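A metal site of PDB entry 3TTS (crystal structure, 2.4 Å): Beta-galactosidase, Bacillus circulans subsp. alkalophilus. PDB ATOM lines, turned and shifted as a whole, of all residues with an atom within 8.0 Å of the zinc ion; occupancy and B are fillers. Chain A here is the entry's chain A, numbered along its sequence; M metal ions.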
ATOM      1  N   ASP A  95     -18.680  26.407  -2.955  1.00  0.00           N
ATOM      2  CA  ASP A  95     -19.093  25.364  -2.031  1.00  0.00           C
ATOM      3  C   ASP A  95     -20.434  25.727  -1.412  1.00  0.00           C
ATOM      4  O   ASP A  95     -21.083  24.941  -0.714  1.00  0.00           O
ATOM      5  CB  ASP A  95     -18.047  25.141  -0.941  1.00  0.00           C
ATOM      6  CG  ASP A  95     -18.014  26.281   0.054  1.00  0.00           C
ATOM      7  OD1 ASP A  95     -17.396  27.335  -0.261  1.00  0.00           O
ATOM      8  OD2 ASP A  95     -18.598  26.154   1.154  1.00  0.00           O
ATOM      9  N   VAL A  96     -20.858  26.949  -1.685  1.00  0.00           N
ATOM     10  CA  VAL A  96     -22.130  27.471  -1.223  1.00  0.00           C
ATOM     11  C   VAL A  96     -23.289  27.005  -2.132  1.00  0.00           C
ATOM     12  O   VAL A  96     -24.441  26.913  -1.700  1.00  0.00           O
ATOM     13  CB  VAL A  96     -22.015  29.005  -1.167  1.00  0.00           C
ATOM     14  CG1 VAL A  96     -22.888  29.701  -2.229  1.00  0.00           C
ATOM     15  CG2 VAL A  96     -22.229  29.507   0.246  1.00  0.00           C
ATOM     16  N   LEU A  97     -22.972  26.694  -3.383  1.00  0.00           N
ATOM     17  CA  LEU A  97     -23.987  26.269  -4.354  1.00  0.00           C
ATOM     18  C   LEU A  97     -24.260  24.778  -4.225  1.00  0.00           C
ATOM     19  O   LEU A  97     -23.377  24.030  -3.818  1.00  0.00           O
ATOM     20  CB  LEU A  97     -23.530  26.600  -5.784  1.00  0.00           C
ATOM     21  CG  LEU A  97     -23.345  28.102  -6.100  1.00  0.00           C
ATOM     22  CD1 LEU A  97     -22.527  28.321  -7.367  1.00  0.00           C
ATOM     23  CD2 LEU A  97     -24.700  28.807  -6.207  1.00  0.00           C
ATOM     24  N   ARG A  98     -25.478  24.365  -4.556  1.00  0.00           N
ATOM     25  CA  ARG A  98     -25.860  22.978  -4.443  1.00  0.00           C
ATOM     26  C   ARG A  98     -25.562  22.148  -5.683  1.00  0.00           C
ATOM     27  O   ARG A  98     -25.428  22.678  -6.777  1.00  0.00           O
ATOM     28  CB  ARG A  98     -27.351  22.861  -4.136  1.00  0.00           C
ATOM     29  CG  ARG A  98     -27.710  23.387  -2.781  1.00  0.00           C
ATOM     30  CD  ARG A  98     -29.188  23.214  -2.485  1.00  0.00           C
ATOM     31  NE  ARG A  98     -29.502  23.682  -1.136  1.00  0.00           N
ATOM     32  CZ  ARG A  98     -30.715  23.666  -0.599  1.00  0.00           C
ATOM     33  NH1 ARG A  98     -31.751  23.210  -1.309  1.00  0.00           N
ATOM     34  NH2 ARG A  98     -30.904  24.119   0.643  1.00  0.00           N
ATOM     35  N   VAL A  99     -25.448  20.830  -5.488  1.00  0.00           N
ATOM     36  CA  VAL A  99     -25.511  19.908  -6.598  1.00  0.00           C
ATOM     37  C   VAL A  99     -26.915  19.290  -6.626  1.00  0.00           C
ATOM     38  O   VAL A  99     -27.411  18.814  -5.599  1.00  0.00           O
ATOM     39  CB  VAL A  99     -24.426  18.836  -6.516  1.00  0.00           C
ATOM     40  CG1 VAL A  99     -24.653  17.747  -7.593  1.00  0.00           C
ATOM     41  CG2 VAL A  99     -23.047  19.481  -6.677  1.00  0.00           C
ATOM     42  N   LYS A 105     -23.832  20.630 -10.734  1.00  0.00           N
ATOM     43  CA  LYS A 105     -23.472  21.770  -9.881  1.00  0.00           C
ATOM     44  C   LYS A 105     -24.243  22.997 -10.364  1.00  0.00           C
ATOM     45  O   LYS A 105     -24.113  23.415 -11.511  1.00  0.00           O
ATOM     46  CB  LYS A 105     -21.963  22.031  -9.972  1.00  0.00           C
ATOM     47  CG  LYS A 105     -21.456  23.234  -9.173  1.00  0.00           C
ATOM     48  CD  LYS A 105     -21.701  23.040  -7.685  1.00  0.00           C
ATOM     49  CE  LYS A 105     -20.723  23.889  -6.856  1.00  0.00           C
ATOM     50  NZ  LYS A 105     -20.749  23.475  -5.419  1.00  0.00           N
ATOM     51  N   ASN A 113     -31.366  27.945  -1.571  1.00  0.00           N
ATOM     52  CA  ASN A 113     -30.609  26.906  -2.231  1.00  0.00           C
ATOM     53  C   ASN A 113     -29.120  26.883  -1.872  1.00  0.00           C
ATOM     54  O   ASN A 113     -28.288  26.472  -2.667  1.00  0.00           O
ATOM     55  CB  ASN A 113     -30.826  26.969  -3.744  1.00  0.00           C
ATOM     56  CG  ASN A 113     -30.532  28.351  -4.314  1.00  0.00           C
ATOM     57  OD1 ASN A 113     -29.858  29.162  -3.672  1.00  0.00           O
ATOM     58  ND2 ASN A 113     -31.010  28.606  -5.514  1.00  0.00           N
ATOM     59  N   SER A 114     -28.804  27.341  -0.664  1.00  0.00           N
ATOM     60  CA  SER A 114     -27.478  27.138  -0.113  1.00  0.00           C
ATOM     61  C   SER A 114     -27.294  25.710   0.339  1.00  0.00           C
ATOM     62  O   SER A 114     -28.213  25.095   0.891  1.00  0.00           O
ATOM     63  CB  SER A 114     -27.216  28.088   1.059  1.00  0.00           C
ATOM     64  OG  SER A 114     -27.131  29.415   0.596  1.00  0.00           O
ATOM     65  N   CYS A 115     -26.112  25.171   0.085  1.00  0.00           N
ATOM     66  CA  CYS A 115     -25.776  23.840   0.575  1.00  0.00           C
ATOM     67  C   CYS A 115     -25.709  23.884   2.095  1.00  0.00           C
ATOM     68  O   CYS A 115     -24.961  24.673   2.658  1.00  0.00           O
ATOM     69  CB  CYS A 115     -24.438  23.378  -0.014  1.00  0.00           C
ATOM     70  SG  CYS A 115     -23.757  21.961   0.887  1.00  0.00           S
ATOM     71  N   PRO A 116     -26.460  23.002   2.766  1.00  0.00           N
ATOM     72  CA  PRO A 116     -26.527  23.135   4.224  1.00  0.00           C
ATOM     73  C   PRO A 116     -25.257  22.600   4.892  1.00  0.00           C
ATOM     74  O   PRO A 116     -25.049  22.847   6.086  1.00  0.00           O
ATOM     75  CB  PRO A 116     -27.751  22.292   4.627  1.00  0.00           C
ATOM     76  CG  PRO A 116     -28.197  21.565   3.345  1.00  0.00           C
ATOM     77  CD  PRO A 116     -27.129  21.771   2.293  1.00  0.00           C
ATOM     78  N   ASN A 117     -24.414  21.914   4.140  1.00  0.00           N
ATOM     79  CA  ASN A 117     -23.132  21.468   4.699  1.00  0.00           C
ATOM     80  C   ASN A 117     -21.953  22.259   4.139  1.00  0.00           C
ATOM     81  O   ASN A 117     -20.823  21.775   4.099  1.00  0.00           O
ATOM     82  CB  ASN A 117     -22.945  19.946   4.538  1.00  0.00           C
ATOM     83  CG  ASN A 117     -23.974  19.151   5.345  1.00  0.00           C
ATOM     84  OD1 ASN A 117     -23.917  19.117   6.563  1.00  0.00           O
ATOM     85  ND2 ASN A 117     -24.918  18.509   4.654  1.00  0.00           N
ATOM     86  N   SER A 118     -22.229  23.488   3.716  1.00  0.00           N
ATOM     87  CA  SER A 118     -21.212  24.392   3.196  1.00  0.00           C
ATOM     88  C   SER A 118     -20.473  25.078   4.333  1.00  0.00           C
ATOM     89  O   SER A 118     -21.086  25.714   5.188  1.00  0.00           O
ATOM     90  CB  SER A 118     -21.863  25.449   2.300  1.00  0.00           C
ATOM     91  OG  SER A 118     -21.014  26.560   2.095  1.00  0.00           O
ATOM     92  N   TYR A 154     -33.119  19.484  -1.609  1.00  0.00           N
ATOM     93  CA  TYR A 154     -32.036  18.601  -1.244  1.00  0.00           C
ATOM     94  C   TYR A 154     -30.758  18.936  -2.008  1.00  0.00           C
ATOM     95  O   TYR A 154     -30.805  19.414  -3.141  1.00  0.00           O
ATOM     96  CB  TYR A 154     -32.425  17.152  -1.545  1.00  0.00           C
ATOM     97  CG  TYR A 154     -33.518  16.624  -0.657  1.00  0.00           C
ATOM     98  CD1 TYR A 154     -33.718  17.148   0.611  1.00  0.00           C
ATOM     99  CD2 TYR A 154     -34.353  15.591  -1.092  1.00  0.00           C
ATOM    100  CE1 TYR A 154     -34.709  16.653   1.437  1.00  0.00           C
ATOM    101  CE2 TYR A 154     -35.354  15.095  -0.269  1.00  0.00           C
ATOM    102  CZ  TYR A 154     -35.521  15.624   0.995  1.00  0.00           C
ATOM    103  OH  TYR A 154     -36.519  15.121   1.811  1.00  0.00           O
ATOM    104  N   CYS A 155     -29.623  18.680  -1.373  1.00  0.00           N
ATOM    105  CA  CYS A 155     -28.328  18.824  -2.025  1.00  0.00           C
ATOM    106  C   CYS A 155     -27.651  17.468  -2.136  1.00  0.00           C
ATOM    107  O   CYS A 155     -27.772  16.628  -1.231  1.00  0.00           O
ATOM    108  CB  CYS A 155     -27.429  19.793  -1.246  1.00  0.00           C
ATOM    109  SG  CYS A 155     -25.846  20.060  -2.052  1.00  0.00           S
ATOM    110  N   TYR A 156     -26.936  17.272  -3.234  1.00  0.00           N
ATOM    111  CA  TYR A 156     -26.242  16.012  -3.474  1.00  0.00           C
ATOM    112  C   TYR A 156     -24.771  16.258  -3.728  1.00  0.00           C
ATOM    113  O   TYR A 156     -24.088  15.426  -4.340  1.00  0.00           O
ATOM    114  CB  TYR A 156     -26.875  15.284  -4.648  1.00  0.00           C
ATOM    115  CG  TYR A 156     -28.329  15.032  -4.411  1.00  0.00           C
ATOM    116  CD1 TYR A 156     -28.754  13.911  -3.692  1.00  0.00           C
ATOM    117  CD2 TYR A 156     -29.296  15.928  -4.870  1.00  0.00           C
ATOM    118  CE1 TYR A 156     -30.110  13.675  -3.466  1.00  0.00           C
ATOM    119  CE2 TYR A 156     -30.653  15.713  -4.651  1.00  0.00           C
ATOM    120  CZ  TYR A 156     -31.052  14.581  -3.939  1.00  0.00           C
ATOM    121  OH  TYR A 156     -32.385  14.348  -3.719  1.00  0.00           O
ATOM    122  N   CYS A 157     -24.252  17.380  -3.231  1.00  0.00           N
ATOM    123  CA  CYS A 157     -22.848  17.710  -3.456  1.00  0.00           C
ATOM    124  C   CYS A 157     -21.886  16.804  -2.669  1.00  0.00           C
ATOM    125  O   CYS A 157     -22.290  16.003  -1.803  1.00  0.00           O
ATOM    126  CB  CYS A 157     -22.558  19.193  -3.168  1.00  0.00           C
ATOM    127  SG  CYS A 157     -22.208  19.580  -1.432  1.00  0.00           S
ATOM    128  N   ASP A 158     -20.606  16.957  -3.004  1.00  0.00           N
ATOM    129  CA  ASP A 158     -19.509  16.257  -2.373  1.00  0.00           C
ATOM    130  C   ASP A 158     -19.488  16.430  -0.848  1.00  0.00           C
ATOM    131  O   ASP A 158     -19.330  15.458  -0.122  1.00  0.00           O
ATOM    132  CB  ASP A 158     -18.189  16.775  -2.951  1.00  0.00           C
ATOM    133  CG  ASP A 158     -17.142  15.711  -3.009  1.00  0.00           C
ATOM    134  OD1 ASP A 158     -17.077  15.014  -4.046  1.00  0.00           O
ATOM    135  OD2 ASP A 158     -16.371  15.567  -2.030  1.00  0.00           O
ATOM    136  N   ASN A 159     -19.622  17.662  -0.383  1.00  0.00           N
ATOM    137  CA  ASN A 159     -19.652  17.936   1.050  1.00  0.00           C
ATOM    138  C   ASN A 159     -20.805  17.230   1.768  1.00  0.00           C
ATOM    139  O   ASN A 159     -20.610  16.687   2.849  1.00  0.00           O
ATOM    140  CB  ASN A 159     -19.693  19.439   1.358  1.00  0.00           C
ATOM    141  CG  ASN A 159     -18.395  20.141   1.027  1.00  0.00           C
ATOM    142  OD1 ASN A 159     -18.376  21.320   0.676  1.00  0.00           O
ATOM    143  ND2 ASN A 159     -17.281  19.405   1.132  1.00  0.00           N
ATOM    144  N   CYS A 160     -22.000  17.265   1.174  1.00  0.00           N
ATOM    145  CA  CYS A 160     -23.142  16.567   1.761  1.00  0.00           C
ATOM    146  C   CYS A 160     -22.894  15.064   1.757  1.00  0.00           C
ATOM    147  O   CYS A 160     -23.304  14.336   2.665  1.00  0.00           O
ATOM    148  CB  CYS A 160     -24.414  16.895   0.989  1.00  0.00           C
ATOM    149  SG  CYS A 160     -25.132  18.505   1.399  1.00  0.00           S
ATOM    150  N   GLU A 161     -22.220  14.592   0.705  1.00  0.00           N
ATOM    151  CA  GLU A 161     -21.929  13.179   0.528  1.00  0.00           C
ATOM    152  C   GLU A 161     -20.955  12.709   1.616  1.00  0.00           C
ATOM    153  O   GLU A 161     -21.161  11.674   2.246  1.00  0.00           O
ATOM    154  CB  GLU A 161     -21.366  12.947  -0.885  1.00  0.00           C
ATOM    155  CG  GLU A 161     -21.271  11.510  -1.317  1.00  0.00           C
ATOM    156  CD  GLU A 161     -21.219  11.342  -2.840  1.00  0.00           C
ATOM    157  OE1 GLU A 161     -22.237  10.887  -3.446  1.00  0.00           O
ATOM    158  OE2 GLU A 161     -20.155  11.654  -3.438  1.00  0.00           O
ATOM    159  N   TYR A 221     -31.083   9.291   3.679  1.00  0.00           N
ATOM    160  CA  TYR A 221     -30.615  10.518   3.057  1.00  0.00           C
ATOM    161  C   TYR A 221     -31.590  11.695   3.253  1.00  0.00           C
ATOM    162  O   TYR A 221     -31.150  12.818   3.482  1.00  0.00           O
ATOM    163  CB  TYR A 221     -30.273  10.320   1.583  1.00  0.00           C
ATOM    164  CG  TYR A 221     -29.366  11.407   1.069  1.00  0.00           C
ATOM    165  CD1 TYR A 221     -28.010  11.394   1.345  1.00  0.00           C
ATOM    166  CD2 TYR A 221     -29.878  12.489   0.348  1.00  0.00           C
ATOM    167  CE1 TYR A 221     -27.176  12.402   0.896  1.00  0.00           C
ATOM    168  CE2 TYR A 221     -29.057  13.494  -0.121  1.00  0.00           C
ATOM    169  CZ  TYR A 221     -27.710  13.458   0.160  1.00  0.00           C
ATOM    170  OH  TYR A 221     -26.903  14.468  -0.305  1.00  0.00           O
ATOM    171  N   PHE A 224     -31.142  12.784   6.764  1.00  0.00           N
ATOM    172  CA  PHE A 224     -29.875  13.485   6.864  1.00  0.00           C
ATOM    173  C   PHE A 224     -29.996  14.904   6.329  1.00  0.00           C
ATOM    174  O   PHE A 224     -29.503  15.851   6.959  1.00  0.00           O
ATOM    175  CB  PHE A 224     -28.792  12.708   6.120  1.00  0.00           C
ATOM    176  CG  PHE A 224     -27.610  13.523   5.726  1.00  0.00           C
ATOM    177  CD1 PHE A 224     -26.754  14.051   6.671  1.00  0.00           C
ATOM    178  CD2 PHE A 224     -27.319  13.733   4.374  1.00  0.00           C
ATOM    179  CE1 PHE A 224     -25.644  14.814   6.297  1.00  0.00           C
ATOM    180  CE2 PHE A 224     -26.203  14.474   3.994  1.00  0.00           C
ATOM    181  CZ  PHE A 224     -25.368  15.015   4.962  1.00  0.00           C
ATOM    182  N   GLN A 225     -30.684  15.044   5.206  1.00  0.00           N
ATOM    183  CA  GLN A 225     -30.890  16.360   4.597  1.00  0.00           C
ATOM    184  C   GLN A 225     -31.797  17.271   5.446  1.00  0.00           C
ATOM    185  O   GLN A 225     -31.551  18.480   5.601  1.00  0.00           O
ATOM    186  CB  GLN A 225     -31.409  16.221   3.160  1.00  0.00           C
ATOM    187  CG  GLN A 225     -30.339  15.792   2.149  1.00  0.00           C
ATOM    188  CD  GLN A 225     -29.437  16.936   1.746  1.00  0.00           C
ATOM    189  OE1 GLN A 225     -29.911  17.956   1.225  1.00  0.00           O
ATOM    190  NE2 GLN A 225     -28.117  16.785   1.980  1.00  0.00           N
ATOM    191  N   SER A 228     -29.631  18.279   8.341  1.00  0.00           N
ATOM    192  CA  SER A 228     -28.607  19.254   7.921  1.00  0.00           C
ATOM    193  C   SER A 228     -29.159  20.671   7.888  1.00  0.00           C
ATOM    194  O   SER A 228     -28.560  21.601   8.436  1.00  0.00           O
ATOM    195  CB  SER A 228     -28.037  18.932   6.533  1.00  0.00           C
ATOM    196  OG  SER A 228     -27.350  17.700   6.545  1.00  0.00           O
HETATM  197 ZN    ZN M   1     -24.415  19.972  -0.313  1.00  0.00          ZN
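The zinc ion is bound by SG of Cys 155 (2.3 Å), SG of Cys 160 (2.4 Å), SG of Cys 115 (2.4 Å) and SG of Cys 157 (2.5 Å). The zinc ion has four donor atoms within binding distance.
Four residues have an atom within 4 Å of the zinc ion: Cys 115, Cys 155, Cys 157 and Cys 160.
SG of Cys 160 sits close to ND2 of Asn 117, at 3.3 Å. OE1 of Gln 225 sits at hydrogen-bond distance from N of Cys 155, 2.7 Å away. SG of Cys 115 lies close to N of Asn 117 (3.3 Å). The backbone NH of Cys 115 lies within hydrogen-bond range of the backbone carbonyl oxygen of Val 96 (3.0 Å). N of Val 99 sits close to SG of Cys 155, at 3.5 Å. SG of Cys 115 lies close to N of Ser 118, 3.6 Å away. The side-chain amide nitrogen (NE2) of Gln 225 sits close to the side-chain sulfur (SG) of Cys 160, 3.5 Å away. OH of Tyr 221 lies within hydrogen-bond range of O of Cys 155 (2.5 Å).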
